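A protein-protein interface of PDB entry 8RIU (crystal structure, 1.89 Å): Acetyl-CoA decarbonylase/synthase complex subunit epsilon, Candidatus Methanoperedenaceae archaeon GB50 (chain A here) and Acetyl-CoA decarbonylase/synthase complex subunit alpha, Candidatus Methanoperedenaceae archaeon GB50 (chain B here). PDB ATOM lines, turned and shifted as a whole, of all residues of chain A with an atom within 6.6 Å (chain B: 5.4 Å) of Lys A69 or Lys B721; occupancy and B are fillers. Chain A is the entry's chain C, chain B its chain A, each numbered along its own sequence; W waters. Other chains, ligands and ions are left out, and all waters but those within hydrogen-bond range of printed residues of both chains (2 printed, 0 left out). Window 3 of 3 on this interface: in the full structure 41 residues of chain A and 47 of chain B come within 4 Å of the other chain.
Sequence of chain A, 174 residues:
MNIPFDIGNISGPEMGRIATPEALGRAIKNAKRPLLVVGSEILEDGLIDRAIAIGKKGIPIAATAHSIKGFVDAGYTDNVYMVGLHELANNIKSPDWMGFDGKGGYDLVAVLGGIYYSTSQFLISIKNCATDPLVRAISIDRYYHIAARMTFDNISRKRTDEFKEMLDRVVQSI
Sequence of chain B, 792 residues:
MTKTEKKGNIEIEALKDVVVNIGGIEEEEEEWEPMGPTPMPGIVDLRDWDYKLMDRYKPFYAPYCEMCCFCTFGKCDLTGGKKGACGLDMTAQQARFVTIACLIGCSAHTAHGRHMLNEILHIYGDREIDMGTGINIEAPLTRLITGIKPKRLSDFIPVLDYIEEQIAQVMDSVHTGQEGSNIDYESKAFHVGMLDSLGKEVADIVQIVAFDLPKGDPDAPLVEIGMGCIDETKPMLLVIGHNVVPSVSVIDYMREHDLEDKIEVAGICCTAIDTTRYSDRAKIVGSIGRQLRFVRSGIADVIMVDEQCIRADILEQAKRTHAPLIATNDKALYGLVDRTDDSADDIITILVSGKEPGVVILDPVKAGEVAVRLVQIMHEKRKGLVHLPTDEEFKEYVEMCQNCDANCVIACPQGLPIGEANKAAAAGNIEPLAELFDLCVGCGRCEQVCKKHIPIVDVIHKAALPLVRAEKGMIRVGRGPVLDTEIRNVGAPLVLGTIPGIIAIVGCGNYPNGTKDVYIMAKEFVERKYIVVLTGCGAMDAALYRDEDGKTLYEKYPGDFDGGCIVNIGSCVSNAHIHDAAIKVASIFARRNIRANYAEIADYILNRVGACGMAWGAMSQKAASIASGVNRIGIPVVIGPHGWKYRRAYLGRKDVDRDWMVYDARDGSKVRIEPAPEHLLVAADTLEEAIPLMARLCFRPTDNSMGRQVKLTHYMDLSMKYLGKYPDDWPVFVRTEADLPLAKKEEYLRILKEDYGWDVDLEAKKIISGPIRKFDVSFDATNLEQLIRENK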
ATOM      1  N   LEU A  43      21.823  21.074  -8.617  1.00  0.00           N
ATOM      2  CA  LEU A  43      20.514  20.451  -8.932  1.00  0.00           C
ATOM      3  C   LEU A  43      19.416  21.173  -8.156  1.00  0.00           C
ATOM      4  O   LEU A  43      18.262  20.744  -8.232  1.00  0.00           O
ATOM      5  CB  LEU A  43      20.589  18.973  -8.551  1.00  0.00           C
ATOM      6  CG  LEU A  43      21.709  18.185  -9.221  1.00  0.00           C
ATOM      7  CD1 LEU A  43      21.830  16.794  -8.624  1.00  0.00           C
ATOM      8  CD2 LEU A  43      21.485  18.103 -10.721  1.00  0.00           C
ATOM      9  N   ILE A  48      21.062  25.178 -12.254  1.00  0.00           N
ATOM     10  CA  ILE A  48      21.591  24.547 -13.459  1.00  0.00           C
ATOM     11  C   ILE A  48      21.332  25.409 -14.688  1.00  0.00           C
ATOM     12  O   ILE A  48      22.074  25.327 -15.676  1.00  0.00           O
ATOM     13  CB  ILE A  48      21.012  23.130 -13.634  1.00  0.00           C
ATOM     14  CG1 ILE A  48      21.924  22.303 -14.546  1.00  0.00           C
ATOM     15  CG2 ILE A  48      19.593  23.170 -14.179  1.00  0.00           C
ATOM     16  CD1 ILE A  48      21.723  20.814 -14.413  1.00  0.00           C
ATOM     17  N   ALA A  63      30.826  17.967 -14.708  1.00  0.00           N
ATOM     18  CA  ALA A  63      29.652  17.668 -13.891  1.00  0.00           C
ATOM     19  C   ALA A  63      30.058  16.621 -12.862  1.00  0.00           C
ATOM     20  O   ALA A  63      30.133  15.429 -13.174  1.00  0.00           O
ATOM     21  CB  ALA A  63      28.495  17.192 -14.767  1.00  0.00           C
ATOM     22  N   HIS A  66      26.603  13.690  -8.807  1.00  0.00           N
ATOM     23  CA  HIS A  66      25.634  13.168  -9.767  1.00  0.00           C
ATOM     24  C   HIS A  66      24.956  14.288 -10.556  1.00  0.00           C
ATOM     25  O   HIS A  66      23.835  14.127 -11.046  1.00  0.00           O
ATOM     26  CB  HIS A  66      24.596  12.291  -9.067  1.00  0.00           C
ATOM     27  CG  HIS A  66      23.747  13.018  -8.073  1.00  0.00           C
ATOM     28  ND1 HIS A  66      24.263  13.583  -6.928  1.00  0.00           N
ATOM     29  CD2 HIS A  66      22.409  13.230  -8.030  1.00  0.00           C
ATOM     30  CE1 HIS A  66      23.282  14.130  -6.229  1.00  0.00           C
ATOM     31  NE2 HIS A  66      22.149  13.931  -6.877  1.00  0.00           N
ATOM     32  N   SER A  67      25.647  15.420 -10.712  1.00  0.00           N
ATOM     33  CA  SER A  67      25.070  16.574 -11.390  1.00  0.00           C
ATOM     34  C   SER A  67      24.739  16.296 -12.852  1.00  0.00           C
ATOM     35  O   SER A  67      23.863  16.965 -13.408  1.00  0.00           O
ATOM     36  CB  SER A  67      26.032  17.756 -11.284  1.00  0.00           C
ATOM     37  OG  SER A  67      27.241  17.470 -11.969  1.00  0.00           O
ATOM     38  N   ILE A  68      25.373  15.308 -13.473  1.00  0.00           N
ATOM     39  CA  ILE A  68      25.097  14.963 -14.904  1.00  0.00           C
ATOM     40  C   ILE A  68      23.598  14.708 -15.121  1.00  0.00           C
ATOM     41  O   ILE A  68      23.099  15.047 -16.193  1.00  0.00           O
ATOM     42  CB  ILE A  68      25.935  13.752 -15.360  1.00  0.00           C
ATOM     43  CG1 ILE A  68      25.803  13.509 -16.865  1.00  0.00           C
ATOM     44  CG2 ILE A  68      25.589  12.514 -14.552  1.00  0.00           C
ATOM     45  CD1 ILE A  68      26.338  14.634 -17.713  1.00  0.00           C
ATOM     46  N   LYS A  69      22.915  14.146 -14.134  1.00  0.00           N
ATOM     47  CA  LYS A  69      21.480  13.797 -14.289  1.00  0.00           C
ATOM     48  C   LYS A  69      20.664  15.051 -14.597  1.00  0.00           C
ATOM     49  O   LYS A  69      19.773  14.979 -15.441  1.00  0.00           O
ATOM     50  CB  LYS A  69      20.964  13.109 -13.024  1.00  0.00           C
ATOM     51  CG  LYS A  69      19.648  12.365 -13.189  1.00  0.00           C
ATOM     52  CD  LYS A  69      19.563  11.111 -12.355  1.00  0.00           C
ATOM     53  CE  LYS A  69      18.608  10.085 -12.924  1.00  0.00           C
ATOM     54  NZ  LYS A  69      18.091   9.179 -11.873  1.00  0.00           N
ATOM     55  N   GLY A  70      20.969  16.155 -13.921  1.00  0.00           N
ATOM     56  CA  GLY A  70      20.239  17.409 -14.152  1.00  0.00           C
ATOM     57  C   GLY A  70      20.496  17.957 -15.540  1.00  0.00           C
ATOM     58  O   GLY A  70      19.591  18.554 -16.111  1.00  0.00           O
ATOM     59  N   PHE A  71      21.700  17.747 -16.058  1.00  0.00           N
ATOM     60  CA  PHE A  71      21.968  18.197 -17.444  1.00  0.00           C
ATOM     61  C   PHE A  71      21.194  17.314 -18.428  1.00  0.00           C
ATOM     62  O   PHE A  71      20.607  17.856 -19.360  1.00  0.00           O
ATOM     63  CB  PHE A  71      23.471  18.209 -17.714  1.00  0.00           C
ATOM     64  CG  PHE A  71      24.218  19.292 -16.978  1.00  0.00           C
ATOM     65  CD1 PHE A  71      24.234  20.590 -17.455  1.00  0.00           C
ATOM     66  CD2 PHE A  71      24.896  19.014 -15.803  1.00  0.00           C
ATOM     67  CE1 PHE A  71      24.918  21.586 -16.779  1.00  0.00           C
ATOM     68  CE2 PHE A  71      25.579  20.010 -15.127  1.00  0.00           C
ATOM     69  CZ  PHE A  71      25.587  21.293 -15.615  1.00  0.00           C
ATOM     70  N   VAL A  72      21.217  16.006 -18.204  1.00  0.00           N
ATOM     71  CA  VAL A  72      20.447  15.059 -19.060  1.00  0.00           C
ATOM     72  C   VAL A  72      18.970  15.446 -18.971  1.00  0.00           C
ATOM     73  O   VAL A  72      18.334  15.594 -20.013  1.00  0.00           O
ATOM     74  CB  VAL A  72      20.696  13.608 -18.618  1.00  0.00           C
ATOM     75  CG1 VAL A  72      19.623  12.666 -19.132  1.00  0.00           C
ATOM     76  CG2 VAL A  72      22.081  13.118 -19.009  1.00  0.00           C
ATOM     77  N   ASP A  73      18.478  15.645 -17.757  1.00  0.00           N
ATOM     78  CA  ASP A  73      17.066  16.045 -17.558  1.00  0.00           C
ATOM     79  C   ASP A  73      16.806  17.407 -18.214  1.00  0.00           C
ATOM     80  O   ASP A  73      15.719  17.584 -18.772  1.00  0.00           O
ATOM     81  CB  ASP A  73      16.702  16.016 -16.076  1.00  0.00           C
ATOM     82  CG  ASP A  73      16.637  14.613 -15.506  1.00  0.00           C
ATOM     83  OD1 ASP A  73      16.930  13.667 -16.255  1.00  0.00           O
ATOM     84  OD2 ASP A  73      16.297  14.482 -14.319  1.00  0.00           O
ATOM     85  N   ALA A  74      17.757  18.336 -18.126  1.00  0.00           N
ATOM     86  CA  ALA A  74      17.547  19.659 -18.701  1.00  0.00           C
ATOM     87  C   ALA A  74      17.677  19.663 -20.216  1.00  0.00           C
ATOM     88  O   ALA A  74      17.254  20.630 -20.860  1.00  0.00           O
ATOM     89  CB  ALA A  74      18.536  20.663 -18.110  1.00  0.00           C
ATOM     90  N   GLU B 524      21.299  -2.121  -2.718  1.00  0.00           N
ATOM     91  CA  GLU B 524      21.470  -2.164  -4.167  1.00  0.00           C
ATOM     92  C   GLU B 524      22.420  -3.281  -4.589  1.00  0.00           C
ATOM     93  O   GLU B 524      22.175  -3.966  -5.590  1.00  0.00           O
ATOM     94  CB  GLU B 524      21.988  -0.813  -4.669  1.00  0.00           C
ATOM     95  CG  GLU B 524      22.180  -0.748  -6.173  1.00  0.00           C
ATOM     96  CD  GLU B 524      20.860  -0.670  -6.910  1.00  0.00           C
ATOM     97  OE1 GLU B 524      20.045   0.216  -6.569  1.00  0.00           O
ATOM     98  OE2 GLU B 524      20.632  -1.500  -7.820  1.00  0.00           O
ATOM     99  N   ARG B 528      21.854  -7.176  -6.473  1.00  0.00           N
ATOM    100  CA  ARG B 528      22.590  -7.540  -7.673  1.00  0.00           C
ATOM    101  C   ARG B 528      23.567  -8.682  -7.427  1.00  0.00           C
ATOM    102  O   ARG B 528      24.460  -8.919  -8.250  1.00  0.00           O
ATOM    103  CB  ARG B 528      23.311  -6.308  -8.232  1.00  0.00           C
ATOM    104  CG  ARG B 528      22.337  -5.303  -8.839  1.00  0.00           C
ATOM    105  CD  ARG B 528      22.971  -3.953  -9.145  1.00  0.00           C
ATOM    106  NE  ARG B 528      21.958  -2.995  -9.573  1.00  0.00           N
ATOM    107  CZ  ARG B 528      21.433  -2.949 -10.790  1.00  0.00           C
ATOM    108  NH1 ARG B 528      21.859  -3.747 -11.757  1.00  0.00           N
ATOM    109  NH2 ARG B 528      20.456  -2.083 -11.044  1.00  0.00           N
ATOM    110  N   MET B 716      26.773  -0.492 -16.081  1.00  0.00           N
ATOM    111  CA  MET B 716      25.992   0.305 -17.061  1.00  0.00           C
ATOM    112  C   MET B 716      24.603   0.616 -16.492  1.00  0.00           C
ATOM    113  O   MET B 716      24.170   1.772 -16.608  1.00  0.00           O
ATOM    114  CB  MET B 716      25.844  -0.462 -18.378  1.00  0.00           C
ATOM    115  CG  MET B 716      27.163  -0.758 -19.057  1.00  0.00           C
ATOM    116  SD  MET B 716      27.892   0.716 -19.804  1.00  0.00           S
ATOM    117  CE  MET B 716      26.763   0.988 -21.168  1.00  0.00           C
ATOM    118  N   ASP B 717      23.937  -0.380 -15.906  1.00  0.00           N
ATOM    119  CA  ASP B 717      22.561  -0.183 -15.384  1.00  0.00           C
ATOM    120  C   ASP B 717      22.607   0.761 -14.180  1.00  0.00           C
ATOM    121  O   ASP B 717      21.742   1.631 -14.071  1.00  0.00           O
ATOM    122  CB  ASP B 717      21.908  -1.522 -15.035  1.00  0.00           C
ATOM    123  CG  ASP B 717      21.683  -2.418 -16.244  1.00  0.00           C
ATOM    124  OD1 ASP B 717      21.889  -1.947 -17.371  1.00  0.00           O
ATOM    125  OD2 ASP B 717      21.329  -3.589 -16.041  1.00  0.00           O
ATOM    126  N   LEU B 718      23.606   0.582 -13.329  1.00  0.00           N
ATOM    127  CA  LEU B 718      23.708   1.454 -12.163  1.00  0.00           C
ATOM    128  C   LEU B 718      24.027   2.885 -12.578  1.00  0.00           C
ATOM    129  O   LEU B 718      23.496   3.841 -11.996  1.00  0.00           O
ATOM    130  CB  LEU B 718      24.767   0.910 -11.203  1.00  0.00           C
ATOM    131  CG  LEU B 718      24.329  -0.276 -10.339  1.00  0.00           C
ATOM    132  CD1 LEU B 718      25.514  -0.836  -9.569  1.00  0.00           C
ATOM    133  CD2 LEU B 718      23.219   0.117  -9.365  1.00  0.00           C
ATOM    134  N   SER B 719      24.880   3.054 -13.594  1.00  0.00           N
ATOM    135  CA  SER B 719      25.171   4.391 -14.098  1.00  0.00           C
ATOM    136  C   SER B 719      23.923   5.055 -14.660  1.00  0.00           C
ATOM    137  O   SER B 719      23.700   6.252 -14.453  1.00  0.00           O
ATOM    138  CB  SER B 719      26.254   4.325 -15.172  1.00  0.00           C
ATOM    139  OG  SER B 719      27.476   3.877 -14.626  1.00  0.00           O
ATOM    140  N   MET B 720      23.107   4.300 -15.394  1.00  0.00           N
ATOM    141  CA  MET B 720      21.893   4.881 -15.955  1.00  0.00           C
ATOM    142  C   MET B 720      20.886   5.182 -14.855  1.00  0.00           C
ATOM    143  O   MET B 720      20.219   6.221 -14.884  1.00  0.00           O
ATOM    144  CB  MET B 720      21.303   3.936 -17.001  1.00  0.00           C
ATOM    145  CG  MET B 720      20.020   4.438 -17.644  1.00  0.00           C
ATOM    146  SD  MET B 720      20.299   5.869 -18.705  1.00  0.00           S
ATOM    147  CE  MET B 720      21.305   5.164 -20.003  1.00  0.00           C
ATOM    148  N   LYS B 721      20.786   4.295 -13.866  1.00  0.00           N
ATOM    149  CA  LYS B 721      19.804   4.465 -12.800  1.00  0.00           C
ATOM    150  C   LYS B 721      20.105   5.699 -11.956  1.00  0.00           C
ATOM    151  O   LYS B 721      19.207   6.496 -11.662  1.00  0.00           O
ATOM    152  CB  LYS B 721      19.784   3.210 -11.931  1.00  0.00           C
ATOM    153  CG  LYS B 721      18.888   3.296 -10.708  1.00  0.00           C
ATOM    154  CD  LYS B 721      18.843   1.958  -9.991  1.00  0.00           C
ATOM    155  CE  LYS B 721      18.007   2.024  -8.726  1.00  0.00           C
ATOM    156  NZ  LYS B 721      18.000   0.703  -8.054  1.00  0.00           N
ATOM    157  N   TYR B 722      21.361   5.870 -11.553  1.00  0.00           N
ATOM    158  CA  TYR B 722      21.730   6.918 -10.610  1.00  0.00           C
ATOM    159  C   TYR B 722      22.235   8.192 -11.269  1.00  0.00           C
ATOM    160  O   TYR B 722      22.073   9.273 -10.693  1.00  0.00           O
ATOM    161  CB  TYR B 722      22.790   6.390  -9.639  1.00  0.00           C
ATOM    162  CG  TYR B 722      22.193   5.483  -8.597  1.00  0.00           C
ATOM    163  CD1 TYR B 722      21.509   6.011  -7.513  1.00  0.00           C
ATOM    164  CD2 TYR B 722      22.280   4.103  -8.709  1.00  0.00           C
ATOM    165  CE1 TYR B 722      20.942   5.192  -6.558  1.00  0.00           C
ATOM    166  CE2 TYR B 722      21.715   3.278  -7.754  1.00  0.00           C
ATOM    167  CZ  TYR B 722      21.046   3.830  -6.684  1.00  0.00           C
ATOM    168  OH  TYR B 722      20.469   3.018  -5.734  1.00  0.00           O
ATOM    169  N   LEU B 723      22.836   8.104 -12.456  1.00  0.00           N
ATOM    170  CA  LEU B 723      23.367   9.280 -13.132  1.00  0.00           C
ATOM    171  C   LEU B 723      22.576   9.672 -14.369  1.00  0.00           C
ATOM    172  O   LEU B 723      22.776  10.778 -14.878  1.00  0.00           O
ATOM    173  CB  LEU B 723      24.838   9.055 -13.525  1.00  0.00           C
ATOM    174  CG  LEU B 723      25.778   8.590 -12.405  1.00  0.00           C
ATOM    175  CD1 LEU B 723      27.142   8.181 -12.955  1.00  0.00           C
ATOM    176  CD2 LEU B 723      25.945   9.675 -11.359  1.00  0.00           C
ATOM    177  N   GLY B 724      21.721   8.787 -14.881  1.00  0.00           N
ATOM    178  CA  GLY B 724      20.852   9.154 -16.014  1.00  0.00           C
ATOM    179  C   GLY B 724      21.541   9.042 -17.359  1.00  0.00           C
ATOM    180  O   GLY B 724      20.936   9.414 -18.369  1.00  0.00           O
HETATM  181  O   HOH W   1      19.850   9.894  -9.351  1.00  0.00           O
HETATM  182  O   HOH W   2      16.274   6.353 -12.294  1.00  0.00           O
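O of Lys B721 lies within hydrogen-bond range of NZ of Lys A69, at 2.9 Å.
O of Leu B723 sits close to N of Lys A69 (3.5 Å).
The side-chain carboxylate of Glu B524 sits at hydrogen-bond distance from the side-chain hydroxyl of Tyr B722.
The backbone NH (N) of Gly B724 is in hydrogen-bond range of the backbone carbonyl oxygen (O) of Ser B719.
The side-chain amino group (NZ) of Lys B721 is in salt-bridge range of the side-chain carboxylate (OE1) of Glu B524, at 2.6 Å.
CB of His A66 touches CD2 of Leu B723 (3.7 Å).
O of Leu B723 touches CG2 of Ile A68 (3.3 Å).
CD of Lys A69 touches O of Tyr B722, at 3.5 Å.
Lys A69 touches Gly B724.
Val A72 touches Gly B724.
Lys A69 touches just these residues of chain B: Lys B721, Tyr B722, Leu B723 and Gly B724.
Lys B721 touches one residue of chain A.
Of the printed residues of chain B, Val A72 touches Gly B724.
Of the printed residues of chain A, Leu B723 touches His A66 (3.7 Å), Ile A68 (3.3 Å) and Lys A69 (3.3 Å).
Of the printed residues of chain A, Gly B724 touches Lys A69 and Val A72.
The nearest residue of chain B that does not touch Lys A69 is Met B720 (4.6 Å).
The nearest printed residue of chain A that does not touch Lys B721 is His A66 (8.3 Å).
Of the 11 printed residues of chain B, 4 touch a printed residue of chain A.
Printed residues of chain B that touch a printed residue of chain A: Lys B721, Tyr B722, Leu B723 and Gly B724.
Along chain B the printed residues that touch a printed residue of chain A span positions 721 to 724.
Printed residues of chain A that touch a printed residue of chain B: His A66, Ile A68, Lys A69 and Val A72.
Hydrophobic or aromatic side chains of chain A within 4 Å of the printed part of chain B: His A66, Ile A68 and Val A72.
Among the printed residues, 7 pairs touch across the chains.
Water W1 lies within hydrogen-bond range of the backbone carbonyl oxygen (O) of Tyr B722 (2.7 Å) and the side-chain amino group (NZ) of Lys A69 (3.2 Å).
Water W2 lies within hydrogen-bond range of O of Lys B721 (3.0 Å) and NZ of Lys A69 (3.4 Å).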
